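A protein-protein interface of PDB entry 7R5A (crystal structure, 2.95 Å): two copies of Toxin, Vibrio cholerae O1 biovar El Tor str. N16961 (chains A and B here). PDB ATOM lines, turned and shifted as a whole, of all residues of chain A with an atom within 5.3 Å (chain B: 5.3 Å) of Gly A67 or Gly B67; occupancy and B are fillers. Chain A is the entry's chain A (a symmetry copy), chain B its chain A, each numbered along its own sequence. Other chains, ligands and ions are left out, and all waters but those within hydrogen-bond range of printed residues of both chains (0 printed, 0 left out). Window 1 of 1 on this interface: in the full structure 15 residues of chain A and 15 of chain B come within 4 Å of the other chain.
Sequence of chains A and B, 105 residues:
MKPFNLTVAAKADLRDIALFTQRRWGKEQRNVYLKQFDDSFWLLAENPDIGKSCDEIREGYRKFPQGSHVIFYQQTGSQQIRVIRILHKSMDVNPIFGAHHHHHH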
ATOM      1  N   TYR A  33     -14.929 -16.960 -11.090  1.00  0.00           N
ATOM      2  CA  TYR A  33     -13.778 -16.196 -10.626  1.00  0.00           C
ATOM      3  C   TYR A  33     -13.161 -16.822  -9.380  1.00  0.00           C
ATOM      4  O   TYR A  33     -11.933 -16.938  -9.272  1.00  0.00           O
ATOM      5  CB  TYR A  33     -14.211 -14.753 -10.363  1.00  0.00           C
ATOM      6  CG  TYR A  33     -13.085 -13.787 -10.101  1.00  0.00           C
ATOM      7  CD1 TYR A  33     -12.419 -13.166 -11.148  1.00  0.00           C
ATOM      8  CD2 TYR A  33     -12.703 -13.479  -8.806  1.00  0.00           C
ATOM      9  CE1 TYR A  33     -11.392 -12.275 -10.911  1.00  0.00           C
ATOM     10  CE2 TYR A  33     -11.684 -12.593  -8.561  1.00  0.00           C
ATOM     11  CZ  TYR A  33     -11.029 -11.992  -9.614  1.00  0.00           C
ATOM     12  OH  TYR A  33     -10.007 -11.103  -9.365  1.00  0.00           O
ATOM     13  N   PRO A  65       0.525 -12.515 -10.240  1.00  0.00           N
ATOM     14  CA  PRO A  65      -0.570 -11.739 -10.832  1.00  0.00           C
ATOM     15  C   PRO A  65      -1.818 -12.607 -11.045  1.00  0.00           C
ATOM     16  O   PRO A  65      -1.671 -13.780 -11.341  1.00  0.00           O
ATOM     17  CB  PRO A  65       0.007 -11.302 -12.185  1.00  0.00           C
ATOM     18  CG  PRO A  65       0.980 -12.405 -12.539  1.00  0.00           C
ATOM     19  CD  PRO A  65       1.572 -12.838 -11.213  1.00  0.00           C
ATOM     20  N   GLN A  66      -3.004 -12.010 -10.890  1.00  0.00           N
ATOM     21  CA  GLN A  66      -4.285 -12.745 -11.067  1.00  0.00           C
ATOM     22  C   GLN A  66      -5.385 -11.760 -11.479  1.00  0.00           C
ATOM     23  O   GLN A  66      -6.158 -11.333 -10.598  1.00  0.00           O
ATOM     24  CB  GLN A  66      -4.660 -13.479  -9.779  1.00  0.00           C
ATOM     25  CG  GLN A  66      -4.747 -14.990  -9.942  1.00  0.00           C
ATOM     26  CD  GLN A  66      -5.892 -15.400 -10.836  1.00  0.00           C
ATOM     27  OE1 GLN A  66      -6.240 -16.576 -10.932  1.00  0.00           O
ATOM     28  NE2 GLN A  66      -6.489 -14.425 -11.501  1.00  0.00           N
ATOM     29  N   GLY A  67      -5.443 -11.418 -12.770  1.00  0.00           N
ATOM     30  CA  GLY A  67      -6.459 -10.482 -13.290  1.00  0.00           C
ATOM     31  C   GLY A  67      -6.122  -9.038 -12.960  1.00  0.00           C
ATOM     32  O   GLY A  67      -5.173  -8.501 -13.565  1.00  0.00           O
ATOM     33  N   SER A  68      -6.872  -8.435 -12.032  1.00  0.00           N
ATOM     34  CA  SER A  68      -6.644  -7.024 -11.625  1.00  0.00           C
ATOM     35  C   SER A  68      -6.069  -6.977 -10.205  1.00  0.00           C
ATOM     36  O   SER A  68      -5.826  -5.862  -9.702  1.00  0.00           O
ATOM     37  CB  SER A  68      -7.916  -6.220 -11.729  1.00  0.00           C
ATOM     38  OG  SER A  68      -7.790  -4.985 -11.041  1.00  0.00           O
ATOM     39  N   HIS A  69      -5.864  -8.147  -9.592  1.00  0.00           N
ATOM     40  CA  HIS A  69      -5.310  -8.231  -8.214  1.00  0.00           C
ATOM     41  C   HIS A  69      -3.963  -8.961  -8.243  1.00  0.00           C
ATOM     42  O   HIS A  69      -3.616  -9.518  -9.303  1.00  0.00           O
ATOM     43  CB  HIS A  69      -6.316  -8.907  -7.272  1.00  0.00           C
ATOM     44  CG  HIS A  69      -7.715  -8.415  -7.435  1.00  0.00           C
ATOM     45  ND1 HIS A  69      -8.556  -8.896  -8.420  1.00  0.00           N
ATOM     46  CD2 HIS A  69      -8.423  -7.493  -6.749  1.00  0.00           C
ATOM     47  CE1 HIS A  69      -9.723  -8.290  -8.333  1.00  0.00           C
ATOM     48  NE2 HIS A  69      -9.668  -7.425  -7.314  1.00  0.00           N
ATOM     49  N   LYS A  89      -3.996  -3.479  -8.170  1.00  0.00           N
ATOM     50  CA  LYS A  89      -2.788  -2.897  -8.821  1.00  0.00           C
ATOM     51  C   LYS A  89      -2.625  -1.597  -7.984  1.00  0.00           C
ATOM     52  O   LYS A  89      -3.079  -0.539  -8.465  1.00  0.00           O
ATOM     53  CB  LYS A  89      -3.013  -2.634 -10.293  1.00  0.00           C
ATOM     54  CG  LYS A  89      -2.173  -3.472 -11.247  1.00  0.00           C
ATOM     55  CD  LYS A  89      -2.993  -4.426 -12.090  1.00  0.00           C
ATOM     56  CE  LYS A  89      -2.958  -4.094 -13.568  1.00  0.00           C
ATOM     57  NZ  LYS A  89      -3.008  -5.314 -14.407  1.00  0.00           N
ATOM     58  N   TYR B  33      -1.333 -17.908 -17.751  1.00  0.00           N
ATOM     59  CA  TYR B  33      -2.341 -16.940 -18.167  1.00  0.00           C
ATOM     60  C   TYR B  33      -3.047 -17.387 -19.443  1.00  0.00           C
ATOM     61  O   TYR B  33      -4.276 -17.294 -19.551  1.00  0.00           O
ATOM     62  CB  TYR B  33      -1.674 -15.577 -18.354  1.00  0.00           C
ATOM     63  CG  TYR B  33      -2.624 -14.426 -18.558  1.00  0.00           C
ATOM     64  CD1 TYR B  33      -3.184 -13.761 -17.476  1.00  0.00           C
ATOM     65  CD2 TYR B  33      -2.944 -13.989 -19.833  1.00  0.00           C
ATOM     66  CE1 TYR B  33      -4.048 -12.701 -17.660  1.00  0.00           C
ATOM     67  CE2 TYR B  33      -3.802 -12.935 -20.025  1.00  0.00           C
ATOM     68  CZ  TYR B  33      -4.354 -12.292 -18.939  1.00  0.00           C
ATOM     69  OH  TYR B  33      -5.214 -11.235 -19.134  1.00  0.00           O
ATOM     70  N   PRO B  65     -15.839 -10.936 -18.289  1.00  0.00           N
ATOM     71  CA  PRO B  65     -14.634 -10.385 -17.662  1.00  0.00           C
ATOM     72  C   PRO B  65     -13.546 -11.457 -17.502  1.00  0.00           C
ATOM     73  O   PRO B  65     -13.887 -12.603 -17.269  1.00  0.00           O
ATOM     74  CB  PRO B  65     -15.137  -9.933 -16.284  1.00  0.00           C
ATOM     75  CG  PRO B  65     -16.280 -10.877 -15.986  1.00  0.00           C
ATOM     76  CD  PRO B  65     -16.929 -11.134 -17.330  1.00  0.00           C
ATOM     77  N   GLN B  66     -12.277 -11.056 -17.629  1.00  0.00           N
ATOM     78  CA  GLN B  66     -11.136 -12.001 -17.498  1.00  0.00           C
ATOM     79  C   GLN B  66      -9.890 -11.234 -17.038  1.00  0.00           C
ATOM     80  O   GLN B  66      -9.054 -10.894 -17.898  1.00  0.00           O
ATOM     81  CB  GLN B  66     -10.881 -12.716 -18.826  1.00  0.00           C
ATOM     82  CG  GLN B  66     -11.046 -14.227 -18.745  1.00  0.00           C
ATOM     83  CD  GLN B  66      -9.988 -14.868 -17.880  1.00  0.00           C
ATOM     84  OE1 GLN B  66      -9.839 -16.088 -17.849  1.00  0.00           O
ATOM     85  NE2 GLN B  66      -9.241 -14.043 -17.165  1.00  0.00           N
ATOM     86  N   GLY B  67      -9.783 -10.977 -15.730  1.00  0.00           N
ATOM     87  CA  GLY B  67      -8.629 -10.250 -15.165  1.00  0.00           C
ATOM     88  C   GLY B  67      -8.722  -8.755 -15.415  1.00  0.00           C
ATOM     89  O   GLY B  67      -9.572  -8.102 -14.778  1.00  0.00           O
ATOM     90  N   SER B  68      -7.878  -8.235 -16.312  1.00  0.00           N
ATOM     91  CA  SER B  68      -7.869  -6.785 -16.641  1.00  0.00           C
ATOM     92  C   SER B  68      -8.422  -6.567 -18.055  1.00  0.00           C
ATOM     93  O   SER B  68      -8.476  -5.402 -18.496  1.00  0.00           O
ATOM     94  CB  SER B  68      -6.482  -6.209 -16.500  1.00  0.00           C
ATOM     95  OG  SER B  68      -6.400  -4.935 -17.120  1.00  0.00           O
ATOM     96  N   HIS B  69      -8.814  -7.653 -18.729  1.00  0.00           N
ATOM     97  CA  HIS B  69      -9.368  -7.569 -20.107  1.00  0.00           C
ATOM     98  C   HIS B  69     -10.818  -8.068 -20.111  1.00  0.00           C
ATOM     99  O   HIS B  69     -11.256  -8.616 -19.081  1.00  0.00           O
ATOM    100  CB  HIS B  69      -8.483  -8.350 -21.089  1.00  0.00           C
ATOM    101  CG  HIS B  69      -7.023  -8.106 -20.905  1.00  0.00           C
ATOM    102  ND1 HIS B  69      -6.277  -8.771 -19.951  1.00  0.00           N
ATOM    103  CD2 HIS B  69      -6.170  -7.277 -21.544  1.00  0.00           C
ATOM    104  CE1 HIS B  69      -5.026  -8.362 -20.011  1.00  0.00           C
ATOM    105  NE2 HIS B  69      -4.933  -7.445 -20.981  1.00  0.00           N
ATOM    106  N   LYS B  89      -9.881  -2.671 -19.888  1.00  0.00           N
ATOM    107  CA  LYS B  89     -10.979  -1.934 -19.201  1.00  0.00           C
ATOM    108  C   LYS B  89     -10.922  -0.582 -19.966  1.00  0.00           C
ATOM    109  O   LYS B  89     -10.302   0.359 -19.431  1.00  0.00           O
ATOM    110  CB  LYS B  89     -10.720  -1.791 -17.718  1.00  0.00           C
ATOM    111  CG  LYS B  89     -11.691  -2.530 -16.806  1.00  0.00           C
ATOM    112  CD  LYS B  89     -11.043  -3.650 -16.020  1.00  0.00           C
ATOM    113  CE  LYS B  89     -11.030  -3.397 -14.527  1.00  0.00           C
ATOM    114  NZ  LYS B  89     -11.186  -4.652 -13.755  1.00  0.00           N
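Gly A67 touches its own counterpart, Gly B67.
Gly A67 touches Ser B68, and with the chains exchanged Ser A68 touches Gly B67.
Positions printed for both chains: 33, 65, 66, 67, 68, 69 and 89.
Of the 3 pairs that touch across the chains among the printed residues, 3 have their exchanged pair printed and touching as well.
Among the printed residues, merely in contact across the chains: Gly A67 with Gly B67, Gly A67 with Ser B68 and Ser A68 with Gly B67.
Pro A65 touches none of the printed residues of chain B.
Gly A67 touches just these residues of chain B: Gly B67 (2.9 Å) and Ser B68 (3.9 Å).
Printed residues of chain B within 4 Å of Ser A68: Gly B67.
Printed residues of chain A within 4 Å of Gly B67: Gly A67 and Ser A68.
Of the printed residues of chain A, Ser B68 touches Gly A67 (3.9 Å).
Lys B89 touches none of the printed residues of chain A.
The nearest residue of chain B that does not touch Gly A67 is Gln B66 (5.1 Å).
The nearest printed residue of chain A that does not touch Ser B68 is Lys A89 (4.2 Å).
Of the 7 printed residues of chain A, 2 touch a printed residue of chain B.
Printed residues of chain B that touch a printed residue of chain A: Gly B67 and Ser B68.
Along chain B the printed residues that touch a printed residue of chain A span positions 67 to 68.
Among the printed residues, 3 pairs touch across the chains.
O of Ser B68 is in hydrogen-bond range of N of Lys B89, at 3.4 Å.
The backbone carbonyl oxygen of Ser A68 sits at hydrogen-bond distance from the backbone NH of Lys A89.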
